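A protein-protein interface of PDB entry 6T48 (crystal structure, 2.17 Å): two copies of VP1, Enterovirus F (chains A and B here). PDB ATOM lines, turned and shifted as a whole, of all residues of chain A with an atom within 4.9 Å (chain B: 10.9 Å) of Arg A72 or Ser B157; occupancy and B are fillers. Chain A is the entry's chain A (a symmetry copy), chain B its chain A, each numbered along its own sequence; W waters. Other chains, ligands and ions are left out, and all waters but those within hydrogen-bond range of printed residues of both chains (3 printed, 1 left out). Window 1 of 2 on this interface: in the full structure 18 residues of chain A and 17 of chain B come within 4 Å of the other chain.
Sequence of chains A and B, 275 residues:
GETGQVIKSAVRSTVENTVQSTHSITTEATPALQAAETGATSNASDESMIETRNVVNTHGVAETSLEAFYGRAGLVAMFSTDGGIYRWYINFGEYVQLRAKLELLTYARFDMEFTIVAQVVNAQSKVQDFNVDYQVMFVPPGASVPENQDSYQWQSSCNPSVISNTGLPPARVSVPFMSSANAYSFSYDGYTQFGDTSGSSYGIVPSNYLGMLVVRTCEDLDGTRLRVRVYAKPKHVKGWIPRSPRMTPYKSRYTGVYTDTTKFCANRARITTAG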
ATOM      1  N   ALA A  68       0.966  -1.864  11.692  1.00  0.00           N
ATOM      2  CA  ALA A  68       1.702  -2.028  10.442  1.00  0.00           C
ATOM      3  C   ALA A  68       0.772  -2.114   9.241  1.00  0.00           C
ATOM      4  O   ALA A  68       1.104  -1.646   8.154  1.00  0.00           O
ATOM      5  CB  ALA A  68       2.569  -3.275  10.512  1.00  0.00           C
ATOM      6  N   PHE A  69      -0.394  -2.716   9.441  1.00  0.00           N
ATOM      7  CA  PHE A  69      -1.368  -2.872   8.370  1.00  0.00           C
ATOM      8  C   PHE A  69      -2.039  -1.543   8.016  1.00  0.00           C
ATOM      9  O   PHE A  69      -2.168  -1.195   6.842  1.00  0.00           O
ATOM     10  CB  PHE A  69      -2.434  -3.889   8.790  1.00  0.00           C
ATOM     11  CG  PHE A  69      -3.413  -4.233   7.701  1.00  0.00           C
ATOM     12  CD1 PHE A  69      -3.102  -5.199   6.750  1.00  0.00           C
ATOM     13  CD2 PHE A  69      -4.645  -3.587   7.625  1.00  0.00           C
ATOM     14  CE1 PHE A  69      -4.007  -5.522   5.736  1.00  0.00           C
ATOM     15  CE2 PHE A  69      -5.557  -3.900   6.616  1.00  0.00           C
ATOM     16  CZ  PHE A  69      -5.237  -4.870   5.669  1.00  0.00           C
ATOM     17  N   TYR A  70      -2.451  -0.798   9.036  1.00  0.00           N
ATOM     18  CA  TYR A  70      -3.145   0.474   8.833  1.00  0.00           C
ATOM     19  C   TYR A  70      -2.267   1.722   8.803  1.00  0.00           C
ATOM     20  O   TYR A  70      -2.652   2.741   8.232  1.00  0.00           O
ATOM     21  CB  TYR A  70      -4.202   0.649   9.923  1.00  0.00           C
ATOM     22  CG  TYR A  70      -5.378  -0.285   9.788  1.00  0.00           C
ATOM     23  CD1 TYR A  70      -6.308  -0.111   8.764  1.00  0.00           C
ATOM     24  CD2 TYR A  70      -5.565  -1.338  10.685  1.00  0.00           C
ATOM     25  CE1 TYR A  70      -7.403  -0.961   8.632  1.00  0.00           C
ATOM     26  CE2 TYR A  70      -6.660  -2.197  10.562  1.00  0.00           C
ATOM     27  CZ  TYR A  70      -7.572  -2.000   9.531  1.00  0.00           C
ATOM     28  OH  TYR A  70      -8.651  -2.840   9.388  1.00  0.00           O
ATOM     29  N   GLY A  71      -1.093   1.626   9.413  1.00  0.00           N
ATOM     30  CA  GLY A  71      -0.188   2.760   9.508  1.00  0.00           C
ATOM     31  C   GLY A  71       0.451   3.399   8.291  1.00  0.00           C
ATOM     32  O   GLY A  71       1.650   3.669   8.305  1.00  0.00           O
ATOM     33  N   ARG A  72      -0.323   3.642   7.242  1.00  0.00           N
ATOM     34  CA  ARG A  72       0.211   4.302   6.057  1.00  0.00           C
ATOM     35  C   ARG A  72      -0.903   5.090   5.383  1.00  0.00           C
ATOM     36  O   ARG A  72      -2.074   4.741   5.491  1.00  0.00           O
ATOM     37  CB  ARG A  72       0.859   3.295   5.096  1.00  0.00           C
ATOM     38  CG  ARG A  72      -0.003   2.132   4.680  1.00  0.00           C
ATOM     39  CD  ARG A  72       0.822   1.158   3.852  1.00  0.00           C
ATOM     40  NE  ARG A  72       1.875   0.523   4.641  1.00  0.00           N
ATOM     41  CZ  ARG A  72       2.835  -0.245   4.134  1.00  0.00           C
ATOM     42  NH1 ARG A  72       2.890  -0.480   2.828  1.00  0.00           N
ATOM     43  NH2 ARG A  72       3.739  -0.795   4.933  1.00  0.00           N
ATOM     44  N   ALA A  73      -0.529   6.164   4.702  1.00  0.00           N
ATOM     45  CA  ALA A  73      -1.498   7.039   4.060  1.00  0.00           C
ATOM     46  C   ALA A  73      -2.211   6.463   2.846  1.00  0.00           C
ATOM     47  O   ALA A  73      -1.632   5.716   2.054  1.00  0.00           O
ATOM     48  CB  ALA A  73      -0.829   8.356   3.689  1.00  0.00           C
ATOM     49  N   GLY A  74      -3.481   6.832   2.722  1.00  0.00           N
ATOM     50  CA  GLY A  74      -4.309   6.399   1.610  1.00  0.00           C
ATOM     51  C   GLY A  74      -5.208   7.560   1.216  1.00  0.00           C
ATOM     52  O   GLY A  74      -5.595   8.358   2.070  1.00  0.00           O
ATOM     53  N   GLN A  97     -10.065   1.651  -1.759  1.00  0.00           N
ATOM     54  CA  GLN A  97      -8.942   0.976  -1.120  1.00  0.00           C
ATOM     55  C   GLN A  97      -8.904   1.103   0.402  1.00  0.00           C
ATOM     56  O   GLN A  97      -8.917   0.093   1.104  1.00  0.00           O
ATOM     57  CB  GLN A  97      -7.617   1.437  -1.735  1.00  0.00           C
ATOM     58  CG  GLN A  97      -7.440   0.988  -3.186  1.00  0.00           C
ATOM     59  CD  GLN A  97      -6.005   1.092  -3.658  1.00  0.00           C
ATOM     60  OE1 GLN A  97      -5.271   1.990  -3.247  1.00  0.00           O
ATOM     61  NE2 GLN A  97      -5.599   0.184  -4.536  1.00  0.00           N
ATOM     62  N   LEU A  98      -8.864   2.324   0.922  1.00  0.00           N
ATOM     63  CA  LEU A  98      -8.832   2.503   2.370  1.00  0.00           C
ATOM     64  C   LEU A  98     -10.133   2.015   2.997  1.00  0.00           C
ATOM     65  O   LEU A  98     -10.132   1.427   4.077  1.00  0.00           O
ATOM     66  CB  LEU A  98      -8.610   3.973   2.734  1.00  0.00           C
ATOM     67  CG  LEU A  98      -8.619   4.281   4.235  1.00  0.00           C
ATOM     68  CD1 LEU A  98      -7.631   3.379   4.959  1.00  0.00           C
ATOM     69  CD2 LEU A  98      -8.268   5.738   4.456  1.00  0.00           C
ATOM     70  N   LYS A 101     -10.152  -1.635   3.681  1.00  0.00           N
ATOM     71  CA  LYS A 101      -9.241  -1.975   4.775  1.00  0.00           C
ATOM     72  C   LYS A 101      -9.913  -1.790   6.131  1.00  0.00           C
ATOM     73  O   LYS A 101      -9.856  -2.669   6.989  1.00  0.00           O
ATOM     74  CB  LYS A 101      -7.981  -1.098   4.734  1.00  0.00           C
ATOM     75  CG  LYS A 101      -7.075  -1.341   3.548  1.00  0.00           C
ATOM     76  CD  LYS A 101      -5.823  -0.466   3.613  1.00  0.00           C
ATOM     77  CE  LYS A 101      -4.919  -0.854   4.777  1.00  0.00           C
ATOM     78  NZ  LYS A 101      -3.664  -0.049   4.774  1.00  0.00           N
ATOM     79  N   ALA A 232      -5.209  10.190   4.338  1.00  0.00           N
ATOM     80  CA  ALA A 232      -5.374   9.958   5.761  1.00  0.00           C
ATOM     81  C   ALA A 232      -4.582   8.723   6.154  1.00  0.00           C
ATOM     82  O   ALA A 232      -4.533   7.745   5.409  1.00  0.00           O
ATOM     83  CB  ALA A 232      -6.845   9.761   6.097  1.00  0.00           C
ATOM     84  N   LYS A 233      -3.956   8.785   7.323  1.00  0.00           N
ATOM     85  CA  LYS A 233      -3.171   7.679   7.838  1.00  0.00           C
ATOM     86  C   LYS A 233      -3.499   7.401   9.304  1.00  0.00           C
ATOM     87  O   LYS A 233      -3.205   8.215  10.181  1.00  0.00           O
ATOM     88  CB  LYS A 233      -1.673   7.976   7.718  1.00  0.00           C
ATOM     89  CG  LYS A 233      -0.807   6.847   8.275  1.00  0.00           C
ATOM     90  CD  LYS A 233       0.677   7.170   8.283  1.00  0.00           C
ATOM     91  CE  LYS A 233       1.049   7.984   9.499  1.00  0.00           C
ATOM     92  NZ  LYS A 233       2.497   8.307   9.499  1.00  0.00           N
ATOM     93  N   PRO A 234      -4.125   6.245   9.589  1.00  0.00           N
ATOM     94  CA  PRO A 234      -4.488   5.857  10.958  1.00  0.00           C
ATOM     95  C   PRO A 234      -3.219   5.656  11.789  1.00  0.00           C
ATOM     96  O   PRO A 234      -2.209   5.181  11.273  1.00  0.00           O
ATOM     97  CB  PRO A 234      -5.243   4.540  10.759  1.00  0.00           C
ATOM     98  CG  PRO A 234      -5.820   4.681   9.387  1.00  0.00           C
ATOM     99  CD  PRO A 234      -4.656   5.272   8.622  1.00  0.00           C
ATOM    100  N   GLN B 135       4.393  11.336  -8.517  1.00  0.00           N
ATOM    101  CA  GLN B 135       4.210  10.243  -7.580  1.00  0.00           C
ATOM    102  C   GLN B 135       4.913   8.991  -8.074  1.00  0.00           C
ATOM    103  O   GLN B 135       4.792   8.613  -9.240  1.00  0.00           O
ATOM    104  CB  GLN B 135       2.719   9.950  -7.401  1.00  0.00           C
ATOM    105  CG  GLN B 135       2.416   8.840  -6.404  1.00  0.00           C
ATOM    106  CD  GLN B 135       0.928   8.560  -6.282  1.00  0.00           C
ATOM    107  OE1 GLN B 135       0.102   9.239  -6.895  1.00  0.00           O
ATOM    108  NE2 GLN B 135       0.579   7.555  -5.487  1.00  0.00           N
ATOM    109  N   VAL B 136       5.662   8.361  -7.179  1.00  0.00           N
ATOM    110  CA  VAL B 136       6.361   7.128  -7.496  1.00  0.00           C
ATOM    111  C   VAL B 136       5.743   6.084  -6.580  1.00  0.00           C
ATOM    112  O   VAL B 136       5.831   6.192  -5.358  1.00  0.00           O
ATOM    113  CB  VAL B 136       7.870   7.232  -7.198  1.00  0.00           C
ATOM    114  CG1 VAL B 136       8.552   5.904  -7.503  1.00  0.00           C
ATOM    115  CG2 VAL B 136       8.485   8.342  -8.028  1.00  0.00           C
ATOM    116  N   MET B 137       5.095   5.087  -7.168  1.00  0.00           N
ATOM    117  CA  MET B 137       4.464   4.045  -6.375  1.00  0.00           C
ATOM    118  C   MET B 137       5.133   2.696  -6.583  1.00  0.00           C
ATOM    119  O   MET B 137       5.390   2.285  -7.716  1.00  0.00           O
ATOM    120  CB  MET B 137       2.973   3.949  -6.717  1.00  0.00           C
ATOM    121  CG  MET B 137       2.238   2.827  -5.989  1.00  0.00           C
ATOM    122  SD  MET B 137       0.435   2.923  -6.191  1.00  0.00           S
ATOM    123  CE  MET B 137       0.266   2.575  -7.979  1.00  0.00           C
ATOM    124  N   PHE B 138       5.431   2.020  -5.478  1.00  0.00           N
ATOM    125  CA  PHE B 138       6.047   0.699  -5.532  1.00  0.00           C
ATOM    126  C   PHE B 138       4.926  -0.331  -5.573  1.00  0.00           C
ATOM    127  O   PHE B 138       4.117  -0.420  -4.650  1.00  0.00           O
ATOM    128  CB  PHE B 138       6.932   0.473  -4.299  1.00  0.00           C
ATOM    129  CG  PHE B 138       7.407  -0.950  -4.137  1.00  0.00           C
ATOM    130  CD1 PHE B 138       8.019  -1.623  -5.189  1.00  0.00           C
ATOM    131  CD2 PHE B 138       7.255  -1.611  -2.922  1.00  0.00           C
ATOM    132  CE1 PHE B 138       8.474  -2.937  -5.034  1.00  0.00           C
ATOM    133  CE2 PHE B 138       7.707  -2.925  -2.755  1.00  0.00           C
ATOM    134  CZ  PHE B 138       8.317  -3.587  -3.814  1.00  0.00           C
ATOM    135  N   VAL B 139       4.868  -1.094  -6.659  1.00  0.00           N
ATOM    136  CA  VAL B 139       3.841  -2.115  -6.818  1.00  0.00           C
ATOM    137  C   VAL B 139       4.469  -3.504  -6.724  1.00  0.00           C
ATOM    138  O   VAL B 139       5.137  -3.958  -7.658  1.00  0.00           O
ATOM    139  CB  VAL B 139       3.135  -1.988  -8.188  1.00  0.00           C
ATOM    140  CG1 VAL B 139       2.004  -3.002  -8.288  1.00  0.00           C
ATOM    141  CG2 VAL B 139       2.604  -0.573  -8.375  1.00  0.00           C
ATOM    142  N   PRO B 140       4.278  -4.192  -5.589  1.00  0.00           N
ATOM    143  CA  PRO B 140       4.842  -5.536  -5.411  1.00  0.00           C
ATOM    144  C   PRO B 140       4.188  -6.516  -6.388  1.00  0.00           C
ATOM    145  O   PRO B 140       3.063  -6.296  -6.837  1.00  0.00           O
ATOM    146  CB  PRO B 140       4.504  -5.862  -3.958  1.00  0.00           C
ATOM    147  CG  PRO B 140       4.436  -4.505  -3.304  1.00  0.00           C
ATOM    148  CD  PRO B 140       3.686  -3.701  -4.334  1.00  0.00           C
ATOM    149  N   ALA B 143       0.162  -7.238  -7.165  1.00  0.00           N
ATOM    150  CA  ALA B 143      -0.709  -6.084  -6.991  1.00  0.00           C
ATOM    151  C   ALA B 143      -1.031  -5.561  -8.389  1.00  0.00           C
ATOM    152  O   ALA B 143      -0.252  -5.747  -9.323  1.00  0.00           O
ATOM    153  CB  ALA B 143      -0.009  -5.011  -6.169  1.00  0.00           C
ATOM    154  N   SER B 144      -2.180  -4.915  -8.532  1.00  0.00           N
ATOM    155  CA  SER B 144      -2.605  -4.383  -9.820  1.00  0.00           C
ATOM    156  C   SER B 144      -1.797  -3.151 -10.232  1.00  0.00           C
ATOM    157  O   SER B 144      -1.634  -2.217  -9.451  1.00  0.00           O
ATOM    158  CB  SER B 144      -4.096  -4.032  -9.754  1.00  0.00           C
ATOM    159  OG  SER B 144      -4.537  -3.450 -10.964  1.00  0.00           O
ATOM    160  N   SER B 151      -5.783   6.189 -12.871  1.00  0.00           N
ATOM    161  CA  SER B 151      -6.415   4.945 -12.428  1.00  0.00           C
ATOM    162  C   SER B 151      -6.541   4.904 -10.901  1.00  0.00           C
ATOM    163  O   SER B 151      -5.819   5.604 -10.189  1.00  0.00           O
ATOM    164  CB  SER B 151      -5.607   3.744 -12.922  1.00  0.00           C
ATOM    165  OG  SER B 151      -5.532   3.734 -14.337  1.00  0.00           O
ATOM    166  N   TYR B 152      -7.451   4.071 -10.402  1.00  0.00           N
ATOM    167  CA  TYR B 152      -7.696   3.958  -8.963  1.00  0.00           C
ATOM    168  C   TYR B 152      -6.506   3.472  -8.131  1.00  0.00           C
ATOM    169  O   TYR B 152      -6.403   3.801  -6.951  1.00  0.00           O
ATOM    170  CB  TYR B 152      -8.892   3.027  -8.707  1.00  0.00           C
ATOM    171  CG  TYR B 152      -8.539   1.557  -8.788  1.00  0.00           C
ATOM    172  CD1 TYR B 152      -8.083   0.867  -7.664  1.00  0.00           C
ATOM    173  CD2 TYR B 152      -8.601   0.871 -10.003  1.00  0.00           C
ATOM    174  CE1 TYR B 152      -7.691  -0.470  -7.748  1.00  0.00           C
ATOM    175  CE2 TYR B 152      -8.208  -0.465 -10.098  1.00  0.00           C
ATOM    176  CZ  TYR B 152      -7.754  -1.127  -8.967  1.00  0.00           C
ATOM    177  OH  TYR B 152      -7.357  -2.443  -9.061  1.00  0.00           O
ATOM    178  N   GLN B 153      -5.611   2.688  -8.728  1.00  0.00           N
ATOM    179  CA  GLN B 153      -4.474   2.169  -7.967  1.00  0.00           C
ATOM    180  C   GLN B 153      -3.609   3.257  -7.346  1.00  0.00           C
ATOM    181  O   GLN B 153      -2.915   3.010  -6.359  1.00  0.00           O
ATOM    182  CB  GLN B 153      -3.604   1.251  -8.832  1.00  0.00           C
ATOM    183  CG  GLN B 153      -4.336   0.019  -9.349  1.00  0.00           C
ATOM    184  CD  GLN B 153      -4.922   0.235 -10.730  1.00  0.00           C
ATOM    185  OE1 GLN B 153      -5.295   1.349 -11.090  1.00  0.00           O
ATOM    186  NE2 GLN B 153      -5.014  -0.834 -11.508  1.00  0.00           N
ATOM    187  N   TRP B 154      -3.653   4.460  -7.910  1.00  0.00           N
ATOM    188  CA  TRP B 154      -2.853   5.555  -7.378  1.00  0.00           C
ATOM    189  C   TRP B 154      -3.309   5.986  -5.985  1.00  0.00           C
ATOM    190  O   TRP B 154      -2.628   6.771  -5.326  1.00  0.00           O
ATOM    191  CB  TRP B 154      -2.867   6.750  -8.337  1.00  0.00           C
ATOM    192  CG  TRP B 154      -2.156   6.477  -9.632  1.00  0.00           C
ATOM    193  CD1 TRP B 154      -2.725   6.301 -10.861  1.00  0.00           C
ATOM    194  CD2 TRP B 154      -0.742   6.335  -9.821  1.00  0.00           C
ATOM    195  NE1 TRP B 154      -1.754   6.059 -11.804  1.00  0.00           N
ATOM    196  CE2 TRP B 154      -0.528   6.073 -11.193  1.00  0.00           C
ATOM    197  CE3 TRP B 154       0.366   6.402  -8.965  1.00  0.00           C
ATOM    198  CZ2 TRP B 154       0.751   5.879 -11.730  1.00  0.00           C
ATOM    199  CZ3 TRP B 154       1.640   6.209  -9.500  1.00  0.00           C
ATOM    200  CH2 TRP B 154       1.818   5.950 -10.872  1.00  0.00           C
ATOM    201  N   GLN B 155      -4.461   5.484  -5.541  1.00  0.00           N
ATOM    202  CA  GLN B 155      -4.958   5.790  -4.197  1.00  0.00           C
ATOM    203  C   GLN B 155      -3.873   5.339  -3.224  1.00  0.00           C
ATOM    204  O   GLN B 155      -3.721   5.896  -2.136  1.00  0.00           O
ATOM    205  CB  GLN B 155      -6.250   5.020  -3.910  1.00  0.00           C
ATOM    206  CG  GLN B 155      -7.490   5.643  -4.513  1.00  0.00           C
ATOM    207  CD  GLN B 155      -8.694   4.730  -4.423  1.00  0.00           C
ATOM    208  OE1 GLN B 155      -8.926   4.085  -3.399  1.00  0.00           O
ATOM    209  NE2 GLN B 155      -9.479   4.682  -5.493  1.00  0.00           N
ATOM    210  N   SER B 156      -3.142   4.304  -3.637  1.00  0.00           N
ATOM    211  CA  SER B 156      -2.020   3.740  -2.886  1.00  0.00           C
ATOM    212  C   SER B 156      -2.241   3.562  -1.381  1.00  0.00           C
ATOM    213  O   SER B 156      -1.392   3.950  -0.585  1.00  0.00           O
ATOM    214  CB  SER B 156      -0.786   4.621  -3.122  1.00  0.00           C
ATOM    215  OG  SER B 156       0.416   3.946  -2.801  1.00  0.00           O
ATOM    216  N   SER B 157      -3.359   2.957  -0.987  1.00  0.00           N
ATOM    217  CA  SER B 157      -3.645   2.771   0.434  1.00  0.00           C
ATOM    218  C   SER B 157      -2.783   1.692   1.098  1.00  0.00           C
ATOM    219  O   SER B 157      -2.670   1.653   2.323  1.00  0.00           O
ATOM    220  CB  SER B 157      -5.120   2.431   0.641  1.00  0.00           C
ATOM    221  OG  SER B 157      -5.389   1.101   0.233  1.00  0.00           O
ATOM    222  N   CYS B 158      -2.192   0.809   0.296  1.00  0.00           N
ATOM    223  CA  CYS B 158      -1.331  -0.246   0.827  1.00  0.00           C
ATOM    224  C   CYS B 158       0.058  -0.188   0.201  1.00  0.00           C
ATOM    225  O   CYS B 158       1.061  -0.327   0.898  1.00  0.00           O
ATOM    226  CB  CYS B 158      -1.954  -1.620   0.589  1.00  0.00           C
ATOM    227  SG  CYS B 158      -3.439  -1.910   1.571  1.00  0.00           S
ATOM    228  N   ASN B 159       0.116   0.004  -1.113  1.00  0.00           N
ATOM    229  CA  ASN B 159       1.397   0.110  -1.805  1.00  0.00           C
ATOM    230  C   ASN B 159       2.103   1.360  -1.290  1.00  0.00           C
ATOM    231  O   ASN B 159       1.468   2.393  -1.072  1.00  0.00           O
ATOM    232  CB  ASN B 159       1.204   0.295  -3.316  1.00  0.00           C
ATOM    233  CG  ASN B 159       0.583  -0.908  -3.995  1.00  0.00           C
ATOM    234  OD1 ASN B 159       0.150  -0.819  -5.144  1.00  0.00           O
ATOM    235  ND2 ASN B 159       0.548  -2.036  -3.303  1.00  0.00           N
ATOM    236  N   PRO B 160       3.419   1.280  -1.062  1.00  0.00           N
ATOM    237  CA  PRO B 160       4.124   2.474  -0.586  1.00  0.00           C
ATOM    238  C   PRO B 160       4.249   3.433  -1.773  1.00  0.00           C
ATOM    239  O   PRO B 160       4.477   3.001  -2.905  1.00  0.00           O
ATOM    240  CB  PRO B 160       5.494   1.934  -0.175  1.00  0.00           C
ATOM    241  CG  PRO B 160       5.217   0.507   0.182  1.00  0.00           C
ATOM    242  CD  PRO B 160       4.252   0.077  -0.898  1.00  0.00           C
ATOM    243  N   SER B 161       4.081   4.725  -1.525  1.00  0.00           N
ATOM    244  CA  SER B 161       4.223   5.726  -2.575  1.00  0.00           C
ATOM    245  C   SER B 161       4.991   6.896  -2.006  1.00  0.00           C
ATOM    246  O   SER B 161       4.999   7.119  -0.797  1.00  0.00           O
ATOM    247  CB  SER B 161       2.861   6.246  -3.065  1.00  0.00           C
ATOM    248  OG  SER B 161       2.320   5.449  -4.100  1.00  0.00           O
ATOM    249  N   VAL B 162       5.658   7.633  -2.877  1.00  0.00           N
ATOM    250  CA  VAL B 162       6.363   8.815  -2.435  1.00  0.00           C
ATOM    251  C   VAL B 162       5.929   9.904  -3.401  1.00  0.00           C
ATOM    252  O   VAL B 162       5.992   9.737  -4.619  1.00  0.00           O
ATOM    253  CB  VAL B 162       7.903   8.632  -2.445  1.00  0.00           C
ATOM    254  CG1 VAL B 162       8.398   8.321  -3.840  1.00  0.00           C
ATOM    255  CG2 VAL B 162       8.564   9.889  -1.911  1.00  0.00           C
ATOM    256  N   ILE B 163       5.431  11.001  -2.849  1.00  0.00           N
ATOM    257  CA  ILE B 163       4.981  12.122  -3.654  1.00  0.00           C
ATOM    258  C   ILE B 163       5.897  13.302  -3.392  1.00  0.00           C
ATOM    259  O   ILE B 163       6.089  13.703  -2.247  1.00  0.00           O
ATOM    260  CB  ILE B 163       3.533  12.521  -3.295  1.00  0.00           C
ATOM    261  CG1 ILE B 163       2.571  11.424  -3.751  1.00  0.00           C
ATOM    262  CG2 ILE B 163       3.180  13.860  -3.935  1.00  0.00           C
ATOM    263  CD1 ILE B 163       1.140  11.657  -3.332  1.00  0.00           C
ATOM    264  N   SER B 174      14.844   4.576   1.972  1.00  0.00           N
ATOM    265  CA  SER B 174      15.642   3.371   2.174  1.00  0.00           C
ATOM    266  C   SER B 174      14.735   2.152   2.081  1.00  0.00           C
ATOM    267  O   SER B 174      13.548   2.231   2.390  1.00  0.00           O
ATOM    268  CB  SER B 174      16.303   3.380   3.559  1.00  0.00           C
ATOM    269  OG  SER B 174      17.340   4.340   3.636  1.00  0.00           O
ATOM    270  N   PRO B 176      14.805  -2.211   2.939  1.00  0.00           N
ATOM    271  CA  PRO B 176      15.571  -3.267   3.604  1.00  0.00           C
ATOM    272  C   PRO B 176      15.923  -4.400   2.644  1.00  0.00           C
ATOM    273  O   PRO B 176      15.614  -4.327   1.455  1.00  0.00           O
ATOM    274  CB  PRO B 176      14.624  -3.714   4.707  1.00  0.00           C
ATOM    275  CG  PRO B 176      13.291  -3.599   4.036  1.00  0.00           C
ATOM    276  CD  PRO B 176      13.380  -2.276   3.307  1.00  0.00           C
ATOM    277  N   MET B 178      15.010  -7.250   1.026  1.00  0.00           N
ATOM    278  CA  MET B 178      13.693  -7.833   0.785  1.00  0.00           C
ATOM    279  C   MET B 178      13.522  -9.205   0.150  1.00  0.00           C
ATOM    280  O   MET B 178      12.398  -9.693   0.057  1.00  0.00           O
ATOM    281  CB  MET B 178      12.871  -6.835  -0.027  1.00  0.00           C
ATOM    282  CG  MET B 178      12.587  -5.540   0.704  1.00  0.00           C
ATOM    283  SD  MET B 178      12.059  -4.268  -0.437  1.00  0.00           S
ATOM    284  CE  MET B 178      10.498  -4.935  -0.986  1.00  0.00           C
ATOM    285  N   ARG B 216       4.028   8.844 -12.232  1.00  0.00           N
ATOM    286  CA  ARG B 216       3.082   9.723 -12.913  1.00  0.00           C
ATOM    287  C   ARG B 216       3.215  11.133 -12.367  1.00  0.00           C
ATOM    288  O   ARG B 216       3.855  11.351 -11.341  1.00  0.00           O
ATOM    289  CB  ARG B 216       1.641   9.277 -12.655  1.00  0.00           C
ATOM    290  CG  ARG B 216       1.181   9.557 -11.223  1.00  0.00           C
ATOM    291  CD  ARG B 216      -0.334   9.551 -11.076  1.00  0.00           C
ATOM    292  NE  ARG B 216      -0.729   9.895  -9.711  1.00  0.00           N
ATOM    293  CZ  ARG B 216      -1.984  10.101  -9.320  1.00  0.00           C
ATOM    294  NH1 ARG B 216      -2.980  10.001 -10.187  1.00  0.00           N
ATOM    295  NH2 ARG B 216      -2.243  10.409  -8.057  1.00  0.00           N
HETATM  296  O   HOH W   1      -2.844   0.474  -5.434  1.00  0.00           O
HETATM  297  O   HOH W   2      -8.232   4.793  -0.662  1.00  0.00           O
HETATM  298  O   HOH W   3      -4.057   3.757   3.837  1.00  0.00           O
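The side-chain amide oxygen (OE1) of Gln A97 is in hydrogen-bond range of the backbone NH (N) of Ser B157 (3.1 Å).
SG of Cys B158 lies close to NZ of Lys A101 (3.7 Å).
OE1 of Gln A97 is in hydrogen-bond range of N of Ser B156 (3.2 Å).
The guanidinium group of Arg A72 sits at hydrogen-bond distance from the backbone carbonyl oxygen of Cys B158 (2.7 Å).
The side-chain amide oxygen (OE1) of Gln B155 lies within hydrogen-bond range of the backbone NH (N) of Gln A97.
NZ of Lys A101 lies within hydrogen-bond range of O of Ser B157 (3.1 Å).
The backbone carbonyl oxygen of Ala A73 sits close to the backbone carbonyl oxygen of Ser B156, at 3.2 Å.
The side-chain hydroxyl of Ser B156 sits at hydrogen-bond distance from the backbone carbonyl oxygen of Asn B159.
OG of Ser B161 lies within hydrogen-bond range of OG of Ser B156.
The backbone carbonyl oxygen of Phe A69 is in hydrogen-bond range of the side-chain amino group of Lys A101 (2.8 Å).
SD of Met B137 is in hydrogen-bond range of OG of Ser B156, 3.5 Å away.
O of Pro B160 sits at hydrogen-bond distance from N of Phe B138, at 2.9 Å.
O of Gly A74 is in hydrogen-bond range of N of Ala A232, 2.9 Å away.
Among the printed residues, merely in contact across the chains: Arg A72 with Ser B157, Arg A72 with Pro B160, Leu A98 with Ser B157, Gly A74 with Gln B155, Gly A74 with Ser B157, Gln A97 with Tyr B152 and Ala A73 with Ser B157.
No residue of chain B comes within 4 Å of Gly A71.
Arg A72 touches three residues of chain B.
Of chain B, only Ser B156 (3.2 Å) and Ser B157 (3.9 Å) come within 4 Å of Ala A73.
Gln A97 touches just these residues of chain B: Tyr B152 (3.9 Å), Gln B155 (3.1 Å), Ser B156 (3.2 Å) and Ser B157 (3.0 Å).
Leu A98 touches one residue of chain B.
No residue of chain B comes within 4 Å of Lys A233.
No residue of chain B comes within 4 Å of Pro A234.
Of the printed residues of chain A, Gln B155 touches Gly A74 and Gln A97.
Of the printed residues of chain A, Ser B156 touches Ala A73 (3.2 Å) and Gln A97 (3.2 Å).
Ser B157 touches just these residues of chain A: Arg A72 (3.6 Å), Ala A73 (3.9 Å), Gly A74 (3.9 Å), Gln A97 (3.0 Å), Leu A98 (3.7 Å) and Lys A101 (3.1 Å).
The nearest residue of chain B that does not touch Arg A72 is Asn B159 (4.6 Å).
Of the 25 printed residues of chain B, 6 touch a printed residue of chain A.
Hydrophobic or aromatic side chains of chain B that line the printed part of chain A: Tyr B152 and Pro B160.
Of the 13 printed residues of chain A, 6 touch a printed residue of chain B.
Among the printed residues, 14 pairs touch across the chains.
No position is printed for both chains.
Of the 14 pairs that touch across the chains among the printed residues, none has its exchanged pair printed and touching as well.
Water W1 lies within hydrogen-bond range of the backbone carbonyl oxygen (O) of Gln B153 (2.7 Å), the side-chain amide nitrogen (NE2) of Gln A97 (2.9 Å) and the side-chain amide oxygen (OD1) of Asn B159 (3.3 Å).
Water W3 lies within hydrogen-bond range of the backbone carbonyl oxygen (O) of Arg A72 (2.8 Å), the backbone carbonyl oxygen (O) of Ser B157 (2.9 Å) and the backbone NH (N) of Gly A74 (3.3 Å).
Water W2 bridges OE1 of Gln B155 (2.9 Å) and N of Leu A98 (3.0 Å).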
